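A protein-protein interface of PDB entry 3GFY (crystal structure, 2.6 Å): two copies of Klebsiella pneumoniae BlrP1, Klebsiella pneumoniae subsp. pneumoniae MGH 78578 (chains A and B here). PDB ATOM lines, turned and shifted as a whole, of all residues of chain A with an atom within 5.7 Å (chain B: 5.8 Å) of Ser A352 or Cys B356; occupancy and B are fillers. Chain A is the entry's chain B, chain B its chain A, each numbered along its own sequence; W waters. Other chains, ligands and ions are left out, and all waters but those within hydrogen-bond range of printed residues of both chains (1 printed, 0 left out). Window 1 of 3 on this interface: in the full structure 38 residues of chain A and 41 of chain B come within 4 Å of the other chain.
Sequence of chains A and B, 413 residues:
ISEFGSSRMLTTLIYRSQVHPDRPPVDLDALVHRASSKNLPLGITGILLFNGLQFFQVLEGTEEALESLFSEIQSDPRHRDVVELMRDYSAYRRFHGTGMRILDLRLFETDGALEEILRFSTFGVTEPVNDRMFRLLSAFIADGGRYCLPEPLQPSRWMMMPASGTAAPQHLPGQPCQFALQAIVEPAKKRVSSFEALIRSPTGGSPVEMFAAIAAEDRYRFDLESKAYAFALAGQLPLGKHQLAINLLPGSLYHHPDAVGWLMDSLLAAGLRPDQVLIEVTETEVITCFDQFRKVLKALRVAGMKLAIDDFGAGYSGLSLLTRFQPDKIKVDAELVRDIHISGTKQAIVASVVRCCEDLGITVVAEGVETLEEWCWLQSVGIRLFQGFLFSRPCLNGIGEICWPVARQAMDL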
ATOM      1  N   TYR A 147      27.567 -17.931   7.244  1.00  0.00           N
ATOM      2  CA  TYR A 147      28.940 -17.525   6.956  1.00  0.00           C
ATOM      3  C   TYR A 147      29.231 -16.123   7.465  1.00  0.00           C
ATOM      4  O   TYR A 147      30.142 -15.448   6.980  1.00  0.00           O
ATOM      5  CB  TYR A 147      29.246 -17.634   5.464  1.00  0.00           C
ATOM      6  CG  TYR A 147      29.256 -19.055   4.966  1.00  0.00           C
ATOM      7  CD1 TYR A 147      30.328 -19.900   5.242  1.00  0.00           C
ATOM      8  CD2 TYR A 147      28.189 -19.560   4.233  1.00  0.00           C
ATOM      9  CE1 TYR A 147      30.339 -21.204   4.796  1.00  0.00           C
ATOM     10  CE2 TYR A 147      28.190 -20.862   3.783  1.00  0.00           C
ATOM     11  CZ  TYR A 147      29.269 -21.680   4.066  1.00  0.00           C
ATOM     12  OH  TYR A 147      29.272 -22.977   3.619  1.00  0.00           O
ATOM     13  N   GLN A 347      34.552 -20.309   0.312  1.00  0.00           N
ATOM     14  CA  GLN A 347      34.008 -20.555   1.647  1.00  0.00           C
ATOM     15  C   GLN A 347      33.052 -21.742   1.669  1.00  0.00           C
ATOM     16  O   GLN A 347      33.114 -22.575   2.574  1.00  0.00           O
ATOM     17  CB  GLN A 347      33.292 -19.316   2.175  1.00  0.00           C
ATOM     18  CG  GLN A 347      34.221 -18.232   2.681  1.00  0.00           C
ATOM     19  CD  GLN A 347      33.510 -16.914   2.896  1.00  0.00           C
ATOM     20  OE1 GLN A 347      32.327 -16.882   3.235  1.00  0.00           O
ATOM     21  NE2 GLN A 347      34.229 -15.817   2.705  1.00  0.00           N
ATOM     22  N   ALA A 348      32.178 -21.816   0.668  1.00  0.00           N
ATOM     23  CA  ALA A 348      31.187 -22.886   0.584  1.00  0.00           C
ATOM     24  C   ALA A 348      31.835 -24.241   0.309  1.00  0.00           C
ATOM     25  O   ALA A 348      31.479 -25.240   0.932  1.00  0.00           O
ATOM     26  CB  ALA A 348      30.140 -22.571  -0.468  1.00  0.00           C
ATOM     27  N   ILE A 349      32.792 -24.262  -0.616  1.00  0.00           N
ATOM     28  CA  ILE A 349      33.511 -25.491  -0.954  1.00  0.00           C
ATOM     29  C   ILE A 349      34.307 -26.038   0.231  1.00  0.00           C
ATOM     30  O   ILE A 349      34.209 -27.220   0.547  1.00  0.00           O
ATOM     31  CB  ILE A 349      34.438 -25.298  -2.180  1.00  0.00           C
ATOM     32  CG1 ILE A 349      33.608 -25.004  -3.431  1.00  0.00           C
ATOM     33  CG2 ILE A 349      35.296 -26.538  -2.407  1.00  0.00           C
ATOM     34  CD1 ILE A 349      34.432 -24.572  -4.611  1.00  0.00           C
ATOM     35  N   VAL A 350      35.072 -25.173   0.891  1.00  0.00           N
ATOM     36  CA  VAL A 350      35.906 -25.585   2.020  1.00  0.00           C
ATOM     37  C   VAL A 350      35.067 -26.090   3.204  1.00  0.00           C
ATOM     38  O   VAL A 350      35.413 -27.098   3.824  1.00  0.00           O
ATOM     39  CB  VAL A 350      36.900 -24.464   2.435  1.00  0.00           C
ATOM     40  CG1 VAL A 350      37.673 -24.837   3.688  1.00  0.00           C
ATOM     41  CG2 VAL A 350      37.867 -24.192   1.300  1.00  0.00           C
ATOM     42  N   ALA A 351      33.958 -25.409   3.491  1.00  0.00           N
ATOM     43  CA  ALA A 351      33.018 -25.853   4.531  1.00  0.00           C
ATOM     44  C   ALA A 351      32.416 -27.218   4.195  1.00  0.00           C
ATOM     45  O   ALA A 351      32.189 -28.042   5.081  1.00  0.00           O
ATOM     46  CB  ALA A 351      31.919 -24.828   4.734  1.00  0.00           C
ATOM     47  N   SER A 352      32.178 -27.446   2.907  1.00  0.00           N
ATOM     48  CA  SER A 352      31.652 -28.714   2.425  1.00  0.00           C
ATOM     49  C   SER A 352      32.676 -29.841   2.541  1.00  0.00           C
ATOM     50  O   SER A 352      32.314 -30.983   2.815  1.00  0.00           O
ATOM     51  CB  SER A 352      31.191 -28.574   0.977  1.00  0.00           C
ATOM     52  OG  SER A 352      30.527 -29.744   0.540  1.00  0.00           O
ATOM     53  N   VAL A 353      33.948 -29.505   2.331  1.00  0.00           N
ATOM     54  CA  VAL A 353      35.057 -30.452   2.482  1.00  0.00           C
ATOM     55  C   VAL A 353      35.263 -30.839   3.953  1.00  0.00           C
ATOM     56  O   VAL A 353      35.451 -32.016   4.266  1.00  0.00           O
ATOM     57  CB  VAL A 353      36.375 -29.897   1.850  1.00  0.00           C
ATOM     58  CG1 VAL A 353      37.577 -30.755   2.215  1.00  0.00           C
ATOM     59  CG2 VAL A 353      36.244 -29.816   0.333  1.00  0.00           C
ATOM     60  N   VAL A 354      35.198 -29.851   4.845  1.00  0.00           N
ATOM     61  CA  VAL A 354      35.387 -30.072   6.280  1.00  0.00           C
ATOM     62  C   VAL A 354      34.348 -31.045   6.836  1.00  0.00           C
ATOM     63  O   VAL A 354      34.700 -32.019   7.512  1.00  0.00           O
ATOM     64  CB  VAL A 354      35.372 -28.734   7.086  1.00  0.00           C
ATOM     65  CG1 VAL A 354      35.207 -28.978   8.590  1.00  0.00           C
ATOM     66  CG2 VAL A 354      36.630 -27.948   6.828  1.00  0.00           C
ATOM     67  N   ARG A 355      33.079 -30.791   6.524  1.00  0.00           N
ATOM     68  CA  ARG A 355      31.981 -31.607   7.030  1.00  0.00           C
ATOM     69  C   ARG A 355      32.041 -33.037   6.498  1.00  0.00           C
ATOM     70  O   ARG A 355      31.839 -33.997   7.249  1.00  0.00           O
ATOM     71  CB  ARG A 355      30.632 -30.963   6.696  1.00  0.00           C
ATOM     72  CG  ARG A 355      29.481 -31.435   7.574  1.00  0.00           C
ATOM     73  CD  ARG A 355      29.733 -31.114   9.041  1.00  0.00           C
ATOM     74  NE  ARG A 355      28.491 -30.843   9.766  1.00  0.00           N
ATOM     75  CZ  ARG A 355      28.428 -30.308  10.983  1.00  0.00           C
ATOM     76  NH1 ARG A 355      29.540 -29.976  11.633  1.00  0.00           N
ATOM     77  NH2 ARG A 355      27.247 -30.098  11.553  1.00  0.00           N
ATOM     78  N   CYS A 356      32.335 -33.167   5.206  1.00  0.00           N
ATOM     79  CA  CYS A 356      32.408 -34.467   4.545  1.00  0.00           C
ATOM     80  C   CYS A 356      33.529 -35.318   5.128  1.00  0.00           C
ATOM     81  O   CYS A 356      33.320 -36.481   5.476  1.00  0.00           O
ATOM     82  CB  CYS A 356      32.598 -34.294   3.036  1.00  0.00           C
ATOM     83  SG  CYS A 356      32.534 -35.830   2.092  1.00  0.00           S
ATOM     84  N   CYS A 357      34.712 -34.719   5.252  1.00  0.00           N
ATOM     85  CA  CYS A 357      35.876 -35.405   5.804  1.00  0.00           C
ATOM     86  C   CYS A 357      35.692 -35.772   7.271  1.00  0.00           C
ATOM     87  O   CYS A 357      36.213 -36.788   7.725  1.00  0.00           O
ATOM     88  CB  CYS A 357      37.128 -34.553   5.645  1.00  0.00           C
ATOM     89  SG  CYS A 357      37.743 -34.381   3.962  1.00  0.00           S
ATOM     90  N   LEU B 322      34.532 -25.559  -9.837  1.00  0.00           N
ATOM     91  CA  LEU B 322      33.434 -24.830  -9.207  1.00  0.00           C
ATOM     92  C   LEU B 322      33.771 -23.370  -8.943  1.00  0.00           C
ATOM     93  O   LEU B 322      32.886 -22.511  -8.934  1.00  0.00           O
ATOM     94  CB  LEU B 322      32.991 -25.509  -7.912  1.00  0.00           C
ATOM     95  CG  LEU B 322      31.707 -26.337  -7.960  1.00  0.00           C
ATOM     96  CD1 LEU B 322      31.433 -26.959  -6.599  1.00  0.00           C
ATOM     97  CD2 LEU B 322      30.526 -25.478  -8.410  1.00  0.00           C
ATOM     98  N   ALA B 351      25.284 -35.489   0.972  1.00  0.00           N
ATOM     99  CA  ALA B 351      24.894 -34.479   1.946  1.00  0.00           C
ATOM    100  C   ALA B 351      25.692 -33.187   1.808  1.00  0.00           C
ATOM    101  O   ALA B 351      25.140 -32.092   1.881  1.00  0.00           O
ATOM    102  CB  ALA B 351      25.017 -35.023   3.349  1.00  0.00           C
ATOM    103  N   SER B 352      26.993 -33.310   1.604  1.00  0.00           N
ATOM    104  CA  SER B 352      27.823 -32.123   1.526  1.00  0.00           C
ATOM    105  C   SER B 352      27.794 -31.485   0.143  1.00  0.00           C
ATOM    106  O   SER B 352      28.010 -30.289   0.012  1.00  0.00           O
ATOM    107  CB  SER B 352      29.250 -32.414   1.993  1.00  0.00           C
ATOM    108  OG  SER B 352      29.839 -33.410   1.195  1.00  0.00           O
ATOM    109  N   VAL B 353      27.511 -32.286  -0.879  1.00  0.00           N
ATOM    110  CA  VAL B 353      27.189 -31.758  -2.207  1.00  0.00           C
ATOM    111  C   VAL B 353      25.929 -30.888  -2.149  1.00  0.00           C
ATOM    112  O   VAL B 353      25.901 -29.797  -2.703  1.00  0.00           O
ATOM    113  CB  VAL B 353      27.063 -32.896  -3.266  1.00  0.00           C
ATOM    114  CG1 VAL B 353      26.133 -32.513  -4.390  1.00  0.00           C
ATOM    115  CG2 VAL B 353      28.421 -33.238  -3.824  1.00  0.00           C
ATOM    116  N   VAL B 354      24.914 -31.372  -1.437  1.00  0.00           N
ATOM    117  CA  VAL B 354      23.649 -30.666  -1.250  1.00  0.00           C
ATOM    118  C   VAL B 354      23.833 -29.356  -0.491  1.00  0.00           C
ATOM    119  O   VAL B 354      23.342 -28.312  -0.915  1.00  0.00           O
ATOM    120  CB  VAL B 354      22.621 -31.569  -0.531  1.00  0.00           C
ATOM    121  CG1 VAL B 354      21.485 -30.764   0.078  1.00  0.00           C
ATOM    122  CG2 VAL B 354      22.084 -32.603  -1.477  1.00  0.00           C
ATOM    123  N   ARG B 355      24.558 -29.422   0.619  1.00  0.00           N
ATOM    124  CA  ARG B 355      24.845 -28.259   1.446  1.00  0.00           C
ATOM    125  C   ARG B 355      25.704 -27.227   0.721  1.00  0.00           C
ATOM    126  O   ARG B 355      25.445 -26.038   0.801  1.00  0.00           O
ATOM    127  CB  ARG B 355      25.500 -28.702   2.757  1.00  0.00           C
ATOM    128  CG  ARG B 355      25.581 -27.642   3.841  1.00  0.00           C
ATOM    129  CD  ARG B 355      24.241 -26.980   4.112  1.00  0.00           C
ATOM    130  NE  ARG B 355      24.094 -26.615   5.516  1.00  0.00           N
ATOM    131  CZ  ARG B 355      23.157 -27.097   6.327  1.00  0.00           C
ATOM    132  NH1 ARG B 355      22.259 -27.962   5.880  1.00  0.00           N
ATOM    133  NH2 ARG B 355      23.107 -26.701   7.589  1.00  0.00           N
ATOM    134  N   CYS B 356      26.712 -27.691  -0.003  1.00  0.00           N
ATOM    135  CA  CYS B 356      27.523 -26.819  -0.844  1.00  0.00           C
ATOM    136  C   CYS B 356      26.703 -26.078  -1.899  1.00  0.00           C
ATOM    137  O   CYS B 356      26.875 -24.887  -2.090  1.00  0.00           O
ATOM    138  CB  CYS B 356      28.639 -27.619  -1.511  1.00  0.00           C
ATOM    139  SG  CYS B 356      29.821 -26.645  -2.405  1.00  0.00           S
ATOM    140  N   CYS B 357      25.807 -26.787  -2.572  1.00  0.00           N
ATOM    141  CA  CYS B 357      24.984 -26.198  -3.621  1.00  0.00           C
ATOM    142  C   CYS B 357      23.915 -25.265  -3.089  1.00  0.00           C
ATOM    143  O   CYS B 357      23.467 -24.374  -3.782  1.00  0.00           O
ATOM    144  CB  CYS B 357      24.335 -27.285  -4.457  1.00  0.00           C
ATOM    145  SG  CYS B 357      25.474 -28.215  -5.419  1.00  0.00           S
ATOM    146  N   GLU B 358      23.503 -25.492  -1.855  1.00  0.00           N
ATOM    147  CA  GLU B 358      22.614 -24.585  -1.150  1.00  0.00           C
ATOM    148  C   GLU B 358      23.296 -23.221  -0.970  1.00  0.00           C
ATOM    149  O   GLU B 358      22.742 -22.189  -1.349  1.00  0.00           O
ATOM    150  CB  GLU B 358      22.233 -25.191   0.200  1.00  0.00           C
ATOM    151  CG  GLU B 358      21.063 -24.527   0.900  1.00  0.00           C
ATOM    152  CD  GLU B 358      20.684 -25.252   2.177  1.00  0.00           C
ATOM    153  OE1 GLU B 358      20.588 -26.499   2.150  1.00  0.00           O
ATOM    154  OE2 GLU B 358      20.486 -24.577   3.210  1.00  0.00           O
ATOM    155  N   ASP B 359      24.511 -23.232  -0.423  1.00  0.00           N
ATOM    156  CA  ASP B 359      25.301 -22.008  -0.233  1.00  0.00           C
ATOM    157  C   ASP B 359      25.658 -21.312  -1.549  1.00  0.00           C
ATOM    158  O   ASP B 359      25.778 -20.084  -1.599  1.00  0.00           O
ATOM    159  CB  ASP B 359      26.588 -22.306   0.533  1.00  0.00           C
ATOM    160  CG  ASP B 359      26.340 -22.999   1.859  1.00  0.00           C
ATOM    161  OD1 ASP B 359      25.245 -22.849   2.441  1.00  0.00           O
ATOM    162  OD2 ASP B 359      27.261 -23.694   2.327  1.00  0.00           O
ATOM    163  N   LEU B 360      25.834 -22.100  -2.606  1.00  0.00           N
ATOM    164  CA  LEU B 360      26.168 -21.557  -3.919  1.00  0.00           C
ATOM    165  C   LEU B 360      24.924 -21.170  -4.711  1.00  0.00           C
ATOM    166  O   LEU B 360      25.018 -20.488  -5.733  1.00  0.00           O
ATOM    167  CB  LEU B 360      27.018 -22.553  -4.710  1.00  0.00           C
ATOM    168  CG  LEU B 360      28.399 -22.868  -4.131  1.00  0.00           C
ATOM    169  CD1 LEU B 360      29.124 -23.909  -4.963  1.00  0.00           C
ATOM    170  CD2 LEU B 360      29.223 -21.607  -4.003  1.00  0.00           C
ATOM    171  N   GLY B 361      23.760 -21.597  -4.225  1.00  0.00           N
ATOM    172  CA  GLY B 361      22.494 -21.330  -4.899  1.00  0.00           C
ATOM    173  C   GLY B 361      22.355 -22.148  -6.169  1.00  0.00           C
ATOM    174  O   GLY B 361      21.842 -21.663  -7.171  1.00  0.00           O
HETATM  175  O   HOH W   1      28.943 -25.559   1.897  1.00  0.00           O
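The backbone carbonyl oxygen of Ser B352 sits at hydrogen-bond distance from the side-chain hydroxyl of Ser A352, 2.6 Å away. The side-chain hydroxyl of Ser B352 sits close to the side-chain sulfur of Cys A356. The side-chain carboxylate (OD2) of Asp B359 sits at hydrogen-bond distance from the side-chain hydroxyl (OH) of Tyr A147 (2.5 Å).
Ala A348 touches Cys B356 (O to SG, 3.98 Å). Ala A348 touches Asp B359. Ala A348 touches Leu B360 (CB to CD2, 3.8 Å). Leu B322 touches Ile A349. OG of Ser A352 touches CB of Cys B356 (3.5 Å).
Printed residues of chain A within 4 Å of Cys B356: Ala A348 and Ser A352. Of the printed residues of chain B, Ala A348 touches Cys B356, Asp B359 and Leu B360. Of the printed residues of chain B, Tyr A147 touches Asp B359 (2.5 Å). Of the printed residues of chain A, Leu B360 touches Ala A348 (3.8 Å). Of the printed residues of chain B, Ile A349 touches Leu B322 (3.7 Å). The nearest printed residue of chain A that does not touch Leu B322 is Ala A348 (7.4 Å).
Of the 12 printed residues of chain B, 5 touch a printed residue of chain A. Of the 12 printed residues of chain A, 5 touch a printed residue of chain B. Along chain A the printed residues that touch a printed residue of chain B span positions 147 to 356. Among the printed residues, 8 pairs touch across the chains.
Ser A352 touches its own counterpart, Ser B352. Ser A352 touches Cys B356, and with the chains exchanged Cys A356 touches Ser B352. Of the 8 pairs that touch across the chains among the printed residues, 3 have their exchanged pair printed and touching as well.
Water W1 lies within hydrogen-bond range of OD2 of Asp B359 (2.5 Å), O of Ala A348 (2.7 Å) and OH of Tyr A147 (3.1 Å).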
